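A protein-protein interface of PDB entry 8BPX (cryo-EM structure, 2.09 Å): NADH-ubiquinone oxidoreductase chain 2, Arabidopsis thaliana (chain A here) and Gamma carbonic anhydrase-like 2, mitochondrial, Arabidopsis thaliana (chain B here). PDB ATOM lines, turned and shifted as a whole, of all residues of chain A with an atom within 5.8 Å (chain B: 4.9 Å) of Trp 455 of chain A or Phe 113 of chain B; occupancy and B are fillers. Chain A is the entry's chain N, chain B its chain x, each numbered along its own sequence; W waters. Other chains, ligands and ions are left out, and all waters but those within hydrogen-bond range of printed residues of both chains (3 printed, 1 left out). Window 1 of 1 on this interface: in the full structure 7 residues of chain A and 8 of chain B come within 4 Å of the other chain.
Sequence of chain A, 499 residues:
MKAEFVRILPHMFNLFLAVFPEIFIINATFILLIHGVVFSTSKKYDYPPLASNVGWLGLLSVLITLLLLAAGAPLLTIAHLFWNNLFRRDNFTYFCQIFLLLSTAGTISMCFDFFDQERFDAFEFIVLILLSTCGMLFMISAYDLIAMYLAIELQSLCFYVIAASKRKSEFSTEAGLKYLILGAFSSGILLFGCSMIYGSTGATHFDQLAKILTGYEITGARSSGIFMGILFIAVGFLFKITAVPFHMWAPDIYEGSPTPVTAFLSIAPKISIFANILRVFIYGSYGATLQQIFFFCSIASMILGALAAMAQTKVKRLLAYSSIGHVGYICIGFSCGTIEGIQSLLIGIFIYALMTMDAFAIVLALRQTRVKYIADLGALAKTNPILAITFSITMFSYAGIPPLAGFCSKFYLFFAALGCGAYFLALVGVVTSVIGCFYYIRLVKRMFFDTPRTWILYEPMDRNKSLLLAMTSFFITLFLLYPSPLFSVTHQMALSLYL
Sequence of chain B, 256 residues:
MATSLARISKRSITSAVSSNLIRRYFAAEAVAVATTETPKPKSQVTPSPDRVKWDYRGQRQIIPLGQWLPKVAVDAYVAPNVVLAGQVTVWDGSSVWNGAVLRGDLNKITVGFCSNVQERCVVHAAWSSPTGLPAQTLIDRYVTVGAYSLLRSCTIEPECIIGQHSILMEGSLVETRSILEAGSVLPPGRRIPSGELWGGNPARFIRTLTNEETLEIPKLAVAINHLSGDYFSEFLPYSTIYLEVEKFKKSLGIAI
O of Pro 452 of chain A is in hydrogen-bond range of NH2 of Arg 141 of chain B. The backbone carbonyl oxygen of Arg 453 of chain A sits at hydrogen-bond distance from the guanidinium group of Arg 141 of chain B, 3.0 Å away. NE1 of Trp 455 of chain A sits close to NH2 of Arg 141 of chain B (3.4 Å). The side-chain carboxylate of Asp 140 of chain B lies within salt-bridge range of the guanidinium group of Arg 453 of chain A (3.99 Å).
The backbone carbonyl oxygen of Val 111 of chain B is in hydrogen-bond range of the backbone NH of Trp 91 of chain B, at 3.1 Å. OG of Ser 115 of chain B sits at hydrogen-bond distance from O of Asp 140 of chain B, 2.5 Å away. O of Phe 113 of chain B sits at hydrogen-bond distance from N of Tyr 142 of chain B (3.0 Å). The backbone carbonyl oxygen (O) of Pro 452 of chain A lies within hydrogen-bond range of the indole nitrogen (NE1) of Trp 455 of chain A. The side-chain hydroxyl (OG) of Ser 115 of chain B sits at hydrogen-bond distance from the backbone NH (N) of Tyr 142 of chain B, 3.3 Å away.
Lys 382 of chain A touches Phe 113 of chain B. NZ of Lys 382 of chain A touches OH of Tyr 142 of chain B, 3.8 Å away. Thr 383 of chain A touches Phe 113 of chain B. Trp 455 of chain A touches Phe 113 of chain B (CZ3 to CD2, 3.6 Å). Tyr 142 of chain B touches Trp 455 of chain A. Leu 457 of chain A touches Trp 91 of chain B.
Of the printed residues of chain B, Lys 382 of chain A touches Phe 113 and Tyr 142. Of chain B, only Phe 113 (3.6 Å), Arg 141 (3.4 Å) and Tyr 142 (3.7 Å) come within 4 Å of Trp 455 of chain A. Of the printed residues of chain B, Leu 457 of chain A touches Trp 91 (3.5 Å). The nearest residue of chain A that does not touch Phe 113 of chain B is Leu 457 of chain A (4.1 Å).
Of the 11 printed residues of chain A, 6 touch a printed residue of chain B. Hydrophobic or aromatic side chains of chain A within 4 Å of the printed part of chain B: Trp 455 and Leu 457. Of the 10 printed residues of chain B, 5 touch a printed residue of chain A. Among the printed residues, Asp or Glu carboxylates within 4 Å of a Lys or Arg side-chain nitrogen of the other chain: Arg 453 of chain A with Asp 140 of chain B.
Water W3 bridges the side-chain carboxylate of Asp 140 of chain B (2.5 Å) and the guanidinium group of Arg 453 of chain A (3.3 Å). Water W1 lies within hydrogen-bond range of OH of Tyr 142 of chain B (2.7 Å) and NZ of Lys 382 of chain A (3.4 Å). Water W2 bridges the guanidinium group of Arg 453 of chain A (2.7 Å) and the side-chain carboxylate of Asp 140 of chain B (3.3 Å).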
ATOM      1  N   GLY A 378      -6.011 -17.880  10.545  1.00  0.00           N
ATOM      2  CA  GLY A 378      -7.199 -18.710  10.652  1.00  0.00           C
ATOM      3  C   GLY A 378      -7.603 -18.930  12.099  1.00  0.00           C
ATOM      4  O   GLY A 378      -6.762 -19.059  12.988  1.00  0.00           O
ATOM      5  N   ALA A 379      -8.918 -18.951  12.332  1.00  0.00           N
ATOM      6  CA  ALA A 379      -9.521 -19.192  13.642  1.00  0.00           C
ATOM      7  C   ALA A 379      -9.166 -18.116  14.672  1.00  0.00           C
ATOM      8  O   ALA A 379      -9.344 -18.330  15.874  1.00  0.00           O
ATOM      9  CB  ALA A 379      -9.144 -20.578  14.182  1.00  0.00           C
ATOM     10  N   LYS A 382     -11.708 -17.149  17.135  1.00  0.00           N
ATOM     11  CA  LYS A 382     -11.919 -18.080  18.235  1.00  0.00           C
ATOM     12  C   LYS A 382     -10.849 -17.936  19.313  1.00  0.00           C
ATOM     13  O   LYS A 382     -11.166 -17.919  20.505  1.00  0.00           O
ATOM     14  CB  LYS A 382     -11.953 -19.519  17.702  1.00  0.00           C
ATOM     15  CG  LYS A 382     -12.971 -19.747  16.589  1.00  0.00           C
ATOM     16  CD  LYS A 382     -14.202 -20.513  17.050  1.00  0.00           C
ATOM     17  CE  LYS A 382     -14.770 -19.997  18.360  1.00  0.00           C
ATOM     18  NZ  LYS A 382     -15.927 -20.810  18.824  1.00  0.00           N
ATOM     19  N   THR A 383      -9.579 -17.829  18.912  1.00  0.00           N
ATOM     20  CA  THR A 383      -8.484 -17.780  19.873  1.00  0.00           C
ATOM     21  C   THR A 383      -8.281 -16.400  20.486  1.00  0.00           C
ATOM     22  O   THR A 383      -7.678 -16.302  21.558  1.00  0.00           O
ATOM     23  CB  THR A 383      -7.184 -18.260  19.217  1.00  0.00           C
ATOM     24  OG1 THR A 383      -6.805 -17.367  18.162  1.00  0.00           O
ATOM     25  CG2 THR A 383      -7.363 -19.659  18.653  1.00  0.00           C
ATOM     26  N   THR A 451     -12.427 -22.731   8.811  1.00  0.00           N
ATOM     27  CA  THR A 451     -12.268 -23.762   9.837  1.00  0.00           C
ATOM     28  C   THR A 451     -11.055 -24.611   9.478  1.00  0.00           C
ATOM     29  O   THR A 451     -11.190 -25.718   8.943  1.00  0.00           O
ATOM     30  CB  THR A 451     -13.531 -24.617   9.967  1.00  0.00           C
ATOM     31  OG1 THR A 451     -13.937 -25.077   8.672  1.00  0.00           O
ATOM     32  CG2 THR A 451     -14.659 -23.806  10.581  1.00  0.00           C
ATOM     33  N   PRO A 452      -9.849 -24.121   9.756  1.00  0.00           N
ATOM     34  CA  PRO A 452      -8.644 -24.878   9.400  1.00  0.00           C
ATOM     35  C   PRO A 452      -8.425 -26.062  10.329  1.00  0.00           C
ATOM     36  O   PRO A 452      -8.914 -26.110  11.457  1.00  0.00           O
ATOM     37  CB  PRO A 452      -7.511 -23.854   9.542  1.00  0.00           C
ATOM     38  CG  PRO A 452      -8.100 -22.657  10.215  1.00  0.00           C
ATOM     39  CD  PRO A 452      -9.544 -22.896  10.512  1.00  0.00           C
ATOM     40  N   ARG A 453      -7.663 -27.034   9.824  1.00  0.00           N
ATOM     41  CA  ARG A 453      -7.352 -28.217  10.619  1.00  0.00           C
ATOM     42  C   ARG A 453      -6.320 -27.906  11.697  1.00  0.00           C
ATOM     43  O   ARG A 453      -6.433 -28.386  12.829  1.00  0.00           O
ATOM     44  CB  ARG A 453      -6.867 -29.344   9.704  1.00  0.00           C
ATOM     45  CG  ARG A 453      -6.247 -30.530  10.424  1.00  0.00           C
ATOM     46  CD  ARG A 453      -7.219 -31.165  11.411  1.00  0.00           C
ATOM     47  NE  ARG A 453      -6.604 -32.267  12.146  1.00  0.00           N
ATOM     48  CZ  ARG A 453      -5.920 -32.130  13.274  1.00  0.00           C
ATOM     49  NH1 ARG A 453      -5.730 -30.943  13.825  1.00  0.00           N
ATOM     50  NH2 ARG A 453      -5.408 -33.210  13.857  1.00  0.00           N
ATOM     51  N   THR A 454      -5.314 -27.101  11.368  1.00  0.00           N
ATOM     52  CA  THR A 454      -4.286 -26.693  12.316  1.00  0.00           C
ATOM     53  C   THR A 454      -4.442 -25.208  12.617  1.00  0.00           C
ATOM     54  O   THR A 454      -4.528 -24.389  11.697  1.00  0.00           O
ATOM     55  CB  THR A 454      -2.883 -26.985  11.772  1.00  0.00           C
ATOM     56  OG1 THR A 454      -2.673 -28.401  11.722  1.00  0.00           O
ATOM     57  CG2 THR A 454      -1.815 -26.359  12.660  1.00  0.00           C
ATOM     58  N   TRP A 455      -4.491 -24.872  13.901  1.00  0.00           N
ATOM     59  CA  TRP A 455      -4.581 -23.492  14.354  1.00  0.00           C
ATOM     60  C   TRP A 455      -3.218 -23.012  14.837  1.00  0.00           C
ATOM     61  O   TRP A 455      -2.381 -23.802  15.276  1.00  0.00           O
ATOM     62  CB  TRP A 455      -5.596 -23.344  15.491  1.00  0.00           C
ATOM     63  CG  TRP A 455      -7.016 -23.687  15.145  1.00  0.00           C
ATOM     64  CD1 TRP A 455      -7.471 -24.274  14.003  1.00  0.00           C
ATOM     65  CD2 TRP A 455      -8.167 -23.468  15.968  1.00  0.00           C
ATOM     66  NE1 TRP A 455      -8.833 -24.431  14.062  1.00  0.00           N
ATOM     67  CE2 TRP A 455      -9.285 -23.943  15.259  1.00  0.00           C
ATOM     68  CE3 TRP A 455      -8.359 -22.910  17.237  1.00  0.00           C
ATOM     69  CZ2 TRP A 455     -10.577 -23.876  15.773  1.00  0.00           C
ATOM     70  CZ3 TRP A 455      -9.643 -22.845  17.745  1.00  0.00           C
ATOM     71  CH2 TRP A 455     -10.736 -23.327  17.013  1.00  0.00           C
ATOM     72  N   ILE A 456      -3.003 -21.704  14.752  1.00  0.00           N
ATOM     73  CA  ILE A 456      -1.848 -21.060  15.364  1.00  0.00           C
ATOM     74  C   ILE A 456      -2.356 -20.230  16.534  1.00  0.00           C
ATOM     75  O   ILE A 456      -3.209 -19.353  16.359  1.00  0.00           O
ATOM     76  CB  ILE A 456      -1.072 -20.192  14.364  1.00  0.00           C
ATOM     77  CG1 ILE A 456      -0.274 -21.075  13.404  1.00  0.00           C
ATOM     78  CG2 ILE A 456      -0.129 -19.250  15.102  1.00  0.00           C
ATOM     79  CD1 ILE A 456      -0.025 -20.437  12.064  1.00  0.00           C
ATOM     80  N   LEU A 457      -1.841 -20.513  17.726  1.00  0.00           N
ATOM     81  CA  LEU A 457      -2.211 -19.776  18.927  1.00  0.00           C
ATOM     82  C   LEU A 457      -1.190 -18.665  19.151  1.00  0.00           C
ATOM     83  O   LEU A 457       0.010 -18.932  19.239  1.00  0.00           O
ATOM     84  CB  LEU A 457      -2.277 -20.712  20.133  1.00  0.00           C
ATOM     85  CG  LEU A 457      -3.060 -22.010  19.904  1.00  0.00           C
ATOM     86  CD1 LEU A 457      -3.138 -22.853  21.172  1.00  0.00           C
ATOM     87  CD2 LEU A 457      -4.450 -21.709  19.371  1.00  0.00           C
ATOM     88  N   TRP B  91      -2.368 -23.975  27.252  1.00  0.00           N
ATOM     89  CA  TRP B  91      -2.718 -22.940  26.290  1.00  0.00           C
ATOM     90  C   TRP B  91      -3.995 -22.200  26.698  1.00  0.00           C
ATOM     91  O   TRP B  91      -4.631 -22.510  27.706  1.00  0.00           O
ATOM     92  CB  TRP B  91      -2.855 -23.549  24.896  1.00  0.00           C
ATOM     93  CG  TRP B  91      -1.541 -23.791  24.226  1.00  0.00           C
ATOM     94  CD1 TRP B  91      -0.909 -24.990  24.074  1.00  0.00           C
ATOM     95  CD2 TRP B  91      -0.688 -22.810  23.623  1.00  0.00           C
ATOM     96  NE1 TRP B  91       0.281 -24.818  23.412  1.00  0.00           N
ATOM     97  CE2 TRP B  91       0.441 -23.488  23.126  1.00  0.00           C
ATOM     98  CE3 TRP B  91      -0.768 -21.423  23.459  1.00  0.00           C
ATOM     99  CZ2 TRP B  91       1.479 -22.828  22.471  1.00  0.00           C
ATOM    100  CZ3 TRP B  91       0.261 -20.770  22.809  1.00  0.00           C
ATOM    101  CH2 TRP B  91       1.371 -21.475  22.322  1.00  0.00           C
ATOM    102  N   ASP B  92      -4.371 -21.209  25.890  1.00  0.00           N
ATOM    103  CA  ASP B  92      -5.494 -20.337  26.213  1.00  0.00           C
ATOM    104  C   ASP B  92      -6.796 -21.118  26.341  1.00  0.00           C
ATOM    105  O   ASP B  92      -7.104 -21.990  25.522  1.00  0.00           O
ATOM    106  CB  ASP B  92      -5.650 -19.253  25.144  1.00  0.00           C
ATOM    107  CG  ASP B  92      -4.544 -18.220  25.192  1.00  0.00           C
ATOM    108  OD1 ASP B  92      -3.816 -18.161  26.206  1.00  0.00           O
ATOM    109  OD2 ASP B  92      -4.409 -17.458  24.214  1.00  0.00           O
ATOM    110  N   VAL B 111      -1.291 -29.052  26.568  1.00  0.00           N
ATOM    111  CA  VAL B 111      -2.744 -29.029  26.708  1.00  0.00           C
ATOM    112  C   VAL B 111      -3.271 -27.921  25.804  1.00  0.00           C
ATOM    113  O   VAL B 111      -2.963 -26.742  26.012  1.00  0.00           O
ATOM    114  CB  VAL B 111      -3.179 -28.816  28.166  1.00  0.00           C
ATOM    115  CG1 VAL B 111      -4.697 -28.884  28.281  1.00  0.00           C
ATOM    116  CG2 VAL B 111      -2.525 -29.847  29.075  1.00  0.00           C
ATOM    117  N   GLY B 112      -4.081 -28.299  24.817  1.00  0.00           N
ATOM    118  CA  GLY B 112      -4.448 -27.407  23.738  1.00  0.00           C
ATOM    119  C   GLY B 112      -5.556 -26.424  24.076  1.00  0.00           C
ATOM    120  O   GLY B 112      -6.078 -26.365  25.188  1.00  0.00           O
ATOM    121  N   PHE B 113      -5.910 -25.632  23.066  1.00  0.00           N
ATOM    122  CA  PHE B 113      -6.897 -24.570  23.216  1.00  0.00           C
ATOM    123  C   PHE B 113      -8.224 -25.126  23.716  1.00  0.00           C
ATOM    124  O   PHE B 113      -8.785 -26.047  23.116  1.00  0.00           O
ATOM    125  CB  PHE B 113      -7.093 -23.858  21.878  1.00  0.00           C
ATOM    126  CG  PHE B 113      -8.177 -22.818  21.896  1.00  0.00           C
ATOM    127  CD1 PHE B 113      -7.956 -21.575  22.462  1.00  0.00           C
ATOM    128  CD2 PHE B 113      -9.422 -23.090  21.353  1.00  0.00           C
ATOM    129  CE1 PHE B 113      -8.956 -20.618  22.478  1.00  0.00           C
ATOM    130  CE2 PHE B 113     -10.422 -22.139  21.368  1.00  0.00           C
ATOM    131  CZ  PHE B 113     -10.189 -20.902  21.932  1.00  0.00           C
ATOM    132  N   CYS B 114      -8.718 -24.559  24.816  1.00  0.00           N
ATOM    133  CA  CYS B 114     -10.034 -24.887  25.366  1.00  0.00           C
ATOM    134  C   CYS B 114     -10.163 -26.368  25.722  1.00  0.00           C
ATOM    135  O   CYS B 114     -11.246 -26.945  25.625  1.00  0.00           O
ATOM    136  CB  CYS B 114     -11.151 -24.472  24.402  1.00  0.00           C
ATOM    137  SG  CYS B 114     -12.673 -23.944  25.210  1.00  0.00           S
ATOM    138  N   SER B 115      -9.067 -26.998  26.130  1.00  0.00           N
ATOM    139  CA  SER B 115      -9.085 -28.384  26.575  1.00  0.00           C
ATOM    140  C   SER B 115      -9.017 -28.448  28.097  1.00  0.00           C
ATOM    141  O   SER B 115      -8.616 -27.497  28.761  1.00  0.00           O
ATOM    142  CB  SER B 115      -7.924 -29.171  25.959  1.00  0.00           C
ATOM    143  OG  SER B 115      -8.131 -29.367  24.573  1.00  0.00           O
ATOM    144  N   ASP B 140      -4.861 -32.081  22.043  1.00  0.00           N
ATOM    145  CA  ASP B 140      -5.209 -31.031  21.093  1.00  0.00           C
ATOM    146  C   ASP B 140      -6.415 -30.237  21.600  1.00  0.00           C
ATOM    147  O   ASP B 140      -6.873 -30.404  22.734  1.00  0.00           O
ATOM    148  CB  ASP B 140      -5.457 -31.630  19.712  1.00  0.00           C
ATOM    149  CG  ASP B 140      -4.905 -30.765  18.591  1.00  0.00           C
ATOM    150  OD1 ASP B 140      -4.945 -29.522  18.709  1.00  0.00           O
ATOM    151  OD2 ASP B 140      -4.436 -31.329  17.584  1.00  0.00           O
ATOM    152  N   ARG B 141      -6.945 -29.363  20.748  1.00  0.00           N
ATOM    153  CA  ARG B 141      -7.992 -28.436  21.149  1.00  0.00           C
ATOM    154  C   ARG B 141      -9.333 -29.143  21.335  1.00  0.00           C
ATOM    155  O   ARG B 141      -9.601 -30.188  20.736  1.00  0.00           O
ATOM    156  CB  ARG B 141      -8.135 -27.322  20.111  1.00  0.00           C
ATOM    157  CG  ARG B 141      -8.567 -27.799  18.730  1.00  0.00           C
ATOM    158  CD  ARG B 141      -8.842 -26.628  17.800  1.00  0.00           C
ATOM    159  NE  ARG B 141      -9.281 -27.063  16.479  1.00  0.00           N
ATOM    160  CZ  ARG B 141      -8.466 -27.440  15.504  1.00  0.00           C
ATOM    161  NH1 ARG B 141      -7.153 -27.448  15.664  1.00  0.00           N
ATOM    162  NH2 ARG B 141      -8.982 -27.818  14.339  1.00  0.00           N
ATOM    163  N   TYR B 142     -10.179 -28.544  22.175  1.00  0.00           N
ATOM    164  CA  TYR B 142     -11.535 -29.034  22.434  1.00  0.00           C
ATOM    165  C   TYR B 142     -11.533 -30.493  22.886  1.00  0.00           C
ATOM    166  O   TYR B 142     -12.371 -31.294  22.471  1.00  0.00           O
ATOM    167  CB  TYR B 142     -12.431 -28.853  21.204  1.00  0.00           C
ATOM    168  CG  TYR B 142     -12.684 -27.413  20.809  1.00  0.00           C
ATOM    169  CD1 TYR B 142     -13.188 -26.500  21.724  1.00  0.00           C
ATOM    170  CD2 TYR B 142     -12.427 -26.973  19.515  1.00  0.00           C
ATOM    171  CE1 TYR B 142     -13.424 -25.184  21.369  1.00  0.00           C
ATOM    172  CE2 TYR B 142     -12.661 -25.658  19.148  1.00  0.00           C
ATOM    173  CZ  TYR B 142     -13.161 -24.769  20.080  1.00  0.00           C
ATOM    174  OH  TYR B 142     -13.394 -23.460  19.725  1.00  0.00           O
HETATM  175  O   HOH W   1     -14.690 -23.610  17.385  1.00  0.00           O
HETATM  176  O   HOH W   2      -4.133 -29.217  15.110  1.00  0.00           O
HETATM  177  O   HOH W   3      -3.803 -33.585  16.763  1.00  0.00           O
